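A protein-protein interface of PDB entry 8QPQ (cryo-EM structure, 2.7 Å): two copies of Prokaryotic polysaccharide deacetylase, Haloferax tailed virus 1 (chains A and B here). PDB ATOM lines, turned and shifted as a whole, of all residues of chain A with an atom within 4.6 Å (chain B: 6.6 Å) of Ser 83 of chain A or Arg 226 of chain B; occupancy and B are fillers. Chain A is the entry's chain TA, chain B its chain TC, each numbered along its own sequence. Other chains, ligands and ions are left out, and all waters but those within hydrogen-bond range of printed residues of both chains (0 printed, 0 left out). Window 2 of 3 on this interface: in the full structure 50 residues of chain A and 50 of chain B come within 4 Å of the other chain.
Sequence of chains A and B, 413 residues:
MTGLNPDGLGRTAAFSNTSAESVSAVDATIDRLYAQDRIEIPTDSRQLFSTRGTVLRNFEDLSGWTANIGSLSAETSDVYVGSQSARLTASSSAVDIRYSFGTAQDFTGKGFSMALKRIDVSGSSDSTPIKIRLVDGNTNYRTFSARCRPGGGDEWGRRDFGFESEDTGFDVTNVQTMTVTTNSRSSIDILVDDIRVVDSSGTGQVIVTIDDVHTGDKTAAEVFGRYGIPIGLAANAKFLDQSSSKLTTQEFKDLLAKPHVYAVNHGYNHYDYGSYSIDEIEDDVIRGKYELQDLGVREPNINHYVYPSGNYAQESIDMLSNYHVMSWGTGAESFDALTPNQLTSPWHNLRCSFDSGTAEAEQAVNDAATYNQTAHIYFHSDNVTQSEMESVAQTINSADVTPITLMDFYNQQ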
ATOM      1  N   ASN A  58      15.231 -13.940 -16.705  1.00  0.00           N
ATOM      2  CA  ASN A  58      15.845 -12.929 -17.541  1.00  0.00           C
ATOM      3  C   ASN A  58      15.519 -13.090 -19.030  1.00  0.00           C
ATOM      4  O   ASN A  58      15.730 -12.150 -19.775  1.00  0.00           O
ATOM      5  CB  ASN A  58      17.333 -12.822 -17.235  1.00  0.00           C
ATOM      6  CG  ASN A  58      18.150 -14.024 -17.651  1.00  0.00           C
ATOM      7  OD1 ASN A  58      17.649 -14.952 -18.278  1.00  0.00           O
ATOM      8  ND2 ASN A  58      19.440 -13.954 -17.387  1.00  0.00           N
ATOM      9  N   GLU A  60      17.286 -14.519 -21.123  1.00  0.00           N
ATOM     10  CA  GLU A  60      18.542 -14.412 -21.869  1.00  0.00           C
ATOM     11  C   GLU A  60      19.023 -15.762 -22.423  1.00  0.00           C
ATOM     12  O   GLU A  60      19.946 -15.788 -23.247  1.00  0.00           O
ATOM     13  CB  GLU A  60      19.611 -13.726 -21.015  1.00  0.00           C
ATOM     14  CG  GLU A  60      19.181 -12.375 -20.443  1.00  0.00           C
ATOM     15  CD  GLU A  60      18.733 -11.332 -21.473  1.00  0.00           C
ATOM     16  OE1 GLU A  60      19.327 -11.291 -22.578  1.00  0.00           O
ATOM     17  OE2 GLU A  60      17.819 -10.524 -21.172  1.00  0.00           O
ATOM     18  N   THR A  76      16.487 -10.845 -30.607  1.00  0.00           N
ATOM     19  CA  THR A  76      17.792 -10.218 -30.454  1.00  0.00           C
ATOM     20  C   THR A  76      17.865  -8.849 -31.136  1.00  0.00           C
ATOM     21  O   THR A  76      18.813  -8.098 -30.890  1.00  0.00           O
ATOM     22  CB  THR A  76      18.888 -11.124 -31.028  1.00  0.00           C
ATOM     23  OG1 THR A  76      18.620 -11.316 -32.417  1.00  0.00           O
ATOM     24  CG2 THR A  76      18.980 -12.459 -30.313  1.00  0.00           C
ATOM     25  N   VAL A  79      15.226  -5.407 -27.644  1.00  0.00           N
ATOM     26  CA  VAL A  79      15.610  -5.935 -26.347  1.00  0.00           C
ATOM     27  C   VAL A  79      15.363  -4.887 -25.271  1.00  0.00           C
ATOM     28  O   VAL A  79      15.905  -3.789 -25.336  1.00  0.00           O
ATOM     29  CB  VAL A  79      17.076  -6.401 -26.357  1.00  0.00           C
ATOM     30  CG1 VAL A  79      17.481  -6.995 -25.021  1.00  0.00           C
ATOM     31  CG2 VAL A  79      17.339  -7.398 -27.470  1.00  0.00           C
ATOM     32  N   VAL A  81      16.167  -5.559 -21.899  1.00  0.00           N
ATOM     33  CA  VAL A  81      17.261  -5.751 -20.955  1.00  0.00           C
ATOM     34  C   VAL A  81      18.147  -6.884 -21.475  1.00  0.00           C
ATOM     35  O   VAL A  81      17.632  -7.883 -21.974  1.00  0.00           O
ATOM     36  CB  VAL A  81      16.691  -6.031 -19.546  1.00  0.00           C
ATOM     37  CG1 VAL A  81      17.576  -6.888 -18.648  1.00  0.00           C
ATOM     38  CG2 VAL A  81      16.375  -4.737 -18.820  1.00  0.00           C
ATOM     39  N   GLY A  82      19.470  -6.731 -21.355  1.00  0.00           N
ATOM     40  CA  GLY A  82      20.406  -7.812 -21.635  1.00  0.00           C
ATOM     41  C   GLY A  82      20.694  -8.003 -23.123  1.00  0.00           C
ATOM     42  O   GLY A  82      20.814  -7.031 -23.865  1.00  0.00           O
ATOM     43  N   SER A  83      20.843  -9.270 -23.531  1.00  0.00           N
ATOM     44  CA  SER A  83      21.211  -9.688 -24.875  1.00  0.00           C
ATOM     45  C   SER A  83      19.984  -9.952 -25.747  1.00  0.00           C
ATOM     46  O   SER A  83      20.075  -9.871 -26.969  1.00  0.00           O
ATOM     47  CB  SER A  83      22.063 -10.923 -24.805  1.00  0.00           C
ATOM     48  OG  SER A  83      23.174 -10.736 -23.947  1.00  0.00           O
ATOM     49  N   GLN A  84      18.846 -10.303 -25.124  1.00  0.00           N
ATOM     50  CA  GLN A  84      17.633 -10.684 -25.839  1.00  0.00           C
ATOM     51  C   GLN A  84      16.376 -10.524 -24.973  1.00  0.00           C
ATOM     52  O   GLN A  84      16.411 -10.396 -23.747  1.00  0.00           O
ATOM     53  CB  GLN A  84      17.765 -12.111 -26.378  1.00  0.00           C
ATOM     54  CG  GLN A  84      17.981 -13.143 -25.271  1.00  0.00           C
ATOM     55  CD  GLN A  84      18.138 -14.549 -25.794  1.00  0.00           C
ATOM     56  OE1 GLN A  84      18.953 -14.817 -26.675  1.00  0.00           O
ATOM     57  NE2 GLN A  84      17.325 -15.464 -25.286  1.00  0.00           N
ATOM     58  N   THR B 219      29.317  -2.888 -24.550  1.00  0.00           N
ATOM     59  CA  THR B 219      29.408  -4.299 -24.191  1.00  0.00           C
ATOM     60  C   THR B 219      29.116  -4.506 -22.703  1.00  0.00           C
ATOM     61  O   THR B 219      28.392  -5.435 -22.346  1.00  0.00           O
ATOM     62  CB  THR B 219      30.695  -4.967 -24.699  1.00  0.00           C
ATOM     63  OG1 THR B 219      30.636  -6.354 -24.355  1.00  0.00           O
ATOM     64  CG2 THR B 219      31.971  -4.390 -24.119  1.00  0.00           C
ATOM     65  N   ALA B 221      27.057  -2.678 -20.813  1.00  0.00           N
ATOM     66  CA  ALA B 221      25.611  -2.566 -20.676  1.00  0.00           C
ATOM     67  C   ALA B 221      24.909  -3.869 -21.074  1.00  0.00           C
ATOM     68  O   ALA B 221      24.028  -4.322 -20.350  1.00  0.00           O
ATOM     69  CB  ALA B 221      25.117  -1.374 -21.459  1.00  0.00           C
ATOM     70  N   GLU B 222      25.334  -4.508 -22.168  1.00  0.00           N
ATOM     71  CA  GLU B 222      24.761  -5.784 -22.575  1.00  0.00           C
ATOM     72  C   GLU B 222      25.017  -6.877 -21.529  1.00  0.00           C
ATOM     73  O   GLU B 222      24.075  -7.562 -21.125  1.00  0.00           O
ATOM     74  CB  GLU B 222      25.273  -6.183 -23.958  1.00  0.00           C
ATOM     75  CG  GLU B 222      24.481  -7.325 -24.560  1.00  0.00           C
ATOM     76  CD  GLU B 222      25.315  -8.294 -25.374  1.00  0.00           C
ATOM     77  OE1 GLU B 222      26.086  -7.824 -26.234  1.00  0.00           O
ATOM     78  OE2 GLU B 222      25.207  -9.514 -25.133  1.00  0.00           O
ATOM     79  N   VAL B 223      26.263  -6.999 -21.047  1.00  0.00           N
ATOM     80  CA  VAL B 223      26.679  -8.003 -20.070  1.00  0.00           C
ATOM     81  C   VAL B 223      25.913  -7.878 -18.749  1.00  0.00           C
ATOM     82  O   VAL B 223      25.257  -8.829 -18.331  1.00  0.00           O
ATOM     83  CB  VAL B 223      28.205  -8.004 -19.863  1.00  0.00           C
ATOM     84  CG1 VAL B 223      28.618  -8.831 -18.652  1.00  0.00           C
ATOM     85  CG2 VAL B 223      28.900  -8.537 -21.102  1.00  0.00           C
ATOM     86  N   PHE B 224      25.987  -6.714 -18.090  1.00  0.00           N
ATOM     87  CA  PHE B 224      25.310  -6.513 -16.813  1.00  0.00           C
ATOM     88  C   PHE B 224      23.789  -6.495 -16.973  1.00  0.00           C
ATOM     89  O   PHE B 224      23.054  -6.896 -16.079  1.00  0.00           O
ATOM     90  CB  PHE B 224      25.824  -5.237 -16.155  1.00  0.00           C
ATOM     91  CG  PHE B 224      27.192  -5.376 -15.534  1.00  0.00           C
ATOM     92  CD1 PHE B 224      27.329  -5.788 -14.214  1.00  0.00           C
ATOM     93  CD2 PHE B 224      28.344  -5.123 -16.275  1.00  0.00           C
ATOM     94  CE1 PHE B 224      28.588  -5.920 -13.639  1.00  0.00           C
ATOM     95  CE2 PHE B 224      29.607  -5.259 -15.701  1.00  0.00           C
ATOM     96  CZ  PHE B 224      29.724  -5.674 -14.386  1.00  0.00           C
ATOM     97  N   GLY B 225      23.330  -6.110 -18.165  1.00  0.00           N
ATOM     98  CA  GLY B 225      21.944  -6.225 -18.571  1.00  0.00           C
ATOM     99  C   GLY B 225      21.416  -7.658 -18.499  1.00  0.00           C
ATOM    100  O   GLY B 225      20.247  -7.814 -18.182  1.00  0.00           O
ATOM    101  N   ARG B 226      22.241  -8.691 -18.733  1.00  0.00           N
ATOM    102  CA  ARG B 226      21.759 -10.076 -18.709  1.00  0.00           C
ATOM    103  C   ARG B 226      21.109 -10.456 -17.371  1.00  0.00           C
ATOM    104  O   ARG B 226      20.213 -11.299 -17.322  1.00  0.00           O
ATOM    105  CB  ARG B 226      22.865 -11.076 -19.062  1.00  0.00           C
ATOM    106  CG  ARG B 226      23.322 -10.959 -20.508  1.00  0.00           C
ATOM    107  CD  ARG B 226      24.582 -11.757 -20.743  1.00  0.00           C
ATOM    108  NE  ARG B 226      25.156 -11.366 -22.021  1.00  0.00           N
ATOM    109  CZ  ARG B 226      26.399 -11.620 -22.407  1.00  0.00           C
ATOM    110  NH1 ARG B 226      26.836 -11.179 -23.572  1.00  0.00           N
ATOM    111  NH2 ARG B 226      27.230 -12.291 -21.636  1.00  0.00           N
ATOM    112  N   TYR B 227      21.531  -9.786 -16.284  1.00  0.00           N
ATOM    113  CA  TYR B 227      21.007 -10.022 -14.945  1.00  0.00           C
ATOM    114  C   TYR B 227      20.372  -8.767 -14.343  1.00  0.00           C
ATOM    115  O   TYR B 227      20.124  -8.702 -13.141  1.00  0.00           O
ATOM    116  CB  TYR B 227      22.099 -10.634 -14.064  1.00  0.00           C
ATOM    117  CG  TYR B 227      22.842 -11.753 -14.749  1.00  0.00           C
ATOM    118  CD1 TYR B 227      22.210 -12.943 -15.097  1.00  0.00           C
ATOM    119  CD2 TYR B 227      24.165 -11.589 -15.128  1.00  0.00           C
ATOM    120  CE1 TYR B 227      22.870 -13.928 -15.813  1.00  0.00           C
ATOM    121  CE2 TYR B 227      24.846 -12.575 -15.835  1.00  0.00           C
ATOM    122  CZ  TYR B 227      24.192 -13.746 -16.187  1.00  0.00           C
ATOM    123  OH  TYR B 227      24.831 -14.739 -16.876  1.00  0.00           O
ATOM    124  N   GLY B 228      20.114  -7.767 -15.191  1.00  0.00           N
ATOM    125  CA  GLY B 228      19.439  -6.520 -14.835  1.00  0.00           C
ATOM    126  C   GLY B 228      20.106  -5.741 -13.701  1.00  0.00           C
ATOM    127  O   GLY B 228      19.412  -5.115 -12.904  1.00  0.00           O
ATOM    128  N   ILE B 229      21.441  -5.816 -13.625  1.00  0.00           N
ATOM    129  CA  ILE B 229      22.238  -5.116 -12.624  1.00  0.00           C
ATOM    130  C   ILE B 229      22.370  -3.658 -13.064  1.00  0.00           C
ATOM    131  O   ILE B 229      22.736  -3.402 -14.203  1.00  0.00           O
ATOM    132  CB  ILE B 229      23.621  -5.794 -12.482  1.00  0.00           C
ATOM    133  CG1 ILE B 229      23.521  -7.256 -12.038  1.00  0.00           C
ATOM    134  CG2 ILE B 229      24.534  -5.021 -11.551  1.00  0.00           C
ATOM    135  CD1 ILE B 229      24.697  -8.118 -12.462  1.00  0.00           C
ATOM    136  N   HIS B 260      18.426  -0.016 -17.022  1.00  0.00           N
ATOM    137  CA  HIS B 260      19.429  -0.310 -16.005  1.00  0.00           C
ATOM    138  C   HIS B 260      20.625   0.655 -16.028  1.00  0.00           C
ATOM    139  O   HIS B 260      21.476   0.592 -15.142  1.00  0.00           O
ATOM    140  CB  HIS B 260      19.866  -1.779 -16.112  1.00  0.00           C
ATOM    141  CG  HIS B 260      20.512  -2.100 -17.414  1.00  0.00           C
ATOM    142  ND1 HIS B 260      21.877  -1.998 -17.631  1.00  0.00           N
ATOM    143  CD2 HIS B 260      19.967  -2.490 -18.585  1.00  0.00           C
ATOM    144  CE1 HIS B 260      22.142  -2.331 -18.879  1.00  0.00           C
ATOM    145  NE2 HIS B 260      20.980  -2.629 -19.487  1.00  0.00           N
ATOM    146  N   GLN B 386      35.519  -8.665 -22.018  1.00  0.00           N
ATOM    147  CA  GLN B 386      34.110  -9.032 -21.911  1.00  0.00           C
ATOM    148  C   GLN B 386      33.885 -10.211 -20.950  1.00  0.00           C
ATOM    149  O   GLN B 386      32.952 -10.192 -20.149  1.00  0.00           O
ATOM    150  CB  GLN B 386      33.473  -9.250 -23.281  1.00  0.00           C
ATOM    151  CG  GLN B 386      31.978  -9.509 -23.177  1.00  0.00           C
ATOM    152  CD  GLN B 386      31.285  -9.727 -24.496  1.00  0.00           C
ATOM    153  OE1 GLN B 386      31.529  -9.021 -25.473  1.00  0.00           O
ATOM    154  NE2 GLN B 386      30.395 -10.706 -24.540  1.00  0.00           N
ATOM    155  N   GLU B 390      31.601 -10.684 -17.544  1.00  0.00           N
ATOM    156  CA  GLU B 390      30.706 -11.825 -17.425  1.00  0.00           C
ATOM    157  C   GLU B 390      30.936 -12.598 -16.121  1.00  0.00           C
ATOM    158  O   GLU B 390      29.973 -13.037 -15.502  1.00  0.00           O
ATOM    159  CB  GLU B 390      30.815 -12.697 -18.670  1.00  0.00           C
ATOM    160  CG  GLU B 390      30.206 -12.023 -19.887  1.00  0.00           C
ATOM    161  CD  GLU B 390      30.467 -12.725 -21.214  1.00  0.00           C
ATOM    162  OE1 GLU B 390      31.172 -13.762 -21.222  1.00  0.00           O
ATOM    163  OE2 GLU B 390      29.926 -12.255 -22.248  1.00  0.00           O
ATOM    164  N   ALA B 393      29.363 -10.269 -13.444  1.00  0.00           N
ATOM    165  CA  ALA B 393      27.916 -10.270 -13.623  1.00  0.00           C
ATOM    166  C   ALA B 393      27.287 -11.576 -13.107  1.00  0.00           C
ATOM    167  O   ALA B 393      26.337 -11.536 -12.330  1.00  0.00           O
ATOM    168  CB  ALA B 393      27.614  -9.977 -15.075  1.00  0.00           C
ATOM    169  N   ASN B 397      24.755 -12.182  -9.956  1.00  0.00           N
ATOM    170  CA  ASN B 397      23.497 -12.881 -10.164  1.00  0.00           C
ATOM    171  C   ASN B 397      23.323 -14.091  -9.235  1.00  0.00           C
ATOM    172  O   ASN B 397      22.211 -14.367  -8.782  1.00  0.00           O
ATOM    173  CB  ASN B 397      23.392 -13.312 -11.621  1.00  0.00           C
ATOM    174  CG  ASN B 397      22.060 -13.943 -11.942  1.00  0.00           C
ATOM    175  OD1 ASN B 397      20.998 -13.435 -11.583  1.00  0.00           O
ATOM    176  ND2 ASN B 397      22.124 -15.067 -12.627  1.00  0.00           N
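The guanidinium group (NE) of Arg 226 of chain B lies within hydrogen-bond range of the side-chain hydroxyl (OG) of Ser 83 of chain A.
The side-chain amide nitrogen of Asn 58 of chain A lies within hydrogen-bond range of the backbone carbonyl oxygen of Arg 226 of chain B.
N of Gly 82 of chain A is in hydrogen-bond range of O of Gly 225 of chain B (3.4 Å).
The side-chain carboxylate of Glu 222 of chain B is in hydrogen-bond range of the side-chain hydroxyl of Ser 83 of chain A (2.7 Å).
No position is printed for both chains.
Printed residues of chain B within 4 Å of Asn 58 of chain A: Arg 226 and Tyr 227.
Thr 76 of chain A touches none of the printed residues of chain B.
Ser 83 of chain A touches two residues of chain B.
Printed residues of chain A within 4 Å of Glu 222 of chain B: Gly 82 and Ser 83.
Of the printed residues of chain A, Tyr 227 of chain B touches Asn 58 (3.7 Å).
The nearest printed residue of chain A that does not touch Arg 226 of chain B is Val 81 of chain A (5.0 Å).
The nearest printed residue of chain B that does not touch Val 81 of chain A is His 260 of chain B (4.2 Å).
ND2 of Asn 58 of chain A touches CD1 of Tyr 227 of chain B (3.7 Å).
Glu 60 of chain A touches Arg 226 of chain B.
Val 81 of chain A touches Gly 225 of chain B.
O of Glu 222 of chain B touches CA of Gly 82 of chain A, 3.7 Å away.
Gly 82 of chain A touches Arg 226 of chain B.
The side-chain carboxylate (OE2) of Glu 222 of chain B lies within salt-bridge range of the guanidinium group (NH1) of Arg 226 of chain B (2.8 Å).
The side-chain amide oxygen of Asn 58 of chain A lies within hydrogen-bond range of the backbone NH of Glu 60 of chain A (2.9 Å).
The side-chain carboxylate (OE1) of Glu 60 of chain A lies within hydrogen-bond range of the backbone NH (N) of Ser 83 of chain A (2.7 Å).
The guanidinium group (NH2) of Arg 226 of chain B lies within salt-bridge range of the side-chain carboxylate (OE2) of Glu 390 of chain B (2.8 Å).
Printed residues of chain A that touch a printed residue of chain B: Asn 58, Glu 60, Val 81, Gly 82 and Ser 83.
Hydrophobic or aromatic side chains of chain A within 4 Å of the printed part of chain B: Val 81.
Among the printed residues, no Asp or Glu carboxylate lies within 4 Å of a Lys or Arg side-chain nitrogen of the other chain.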
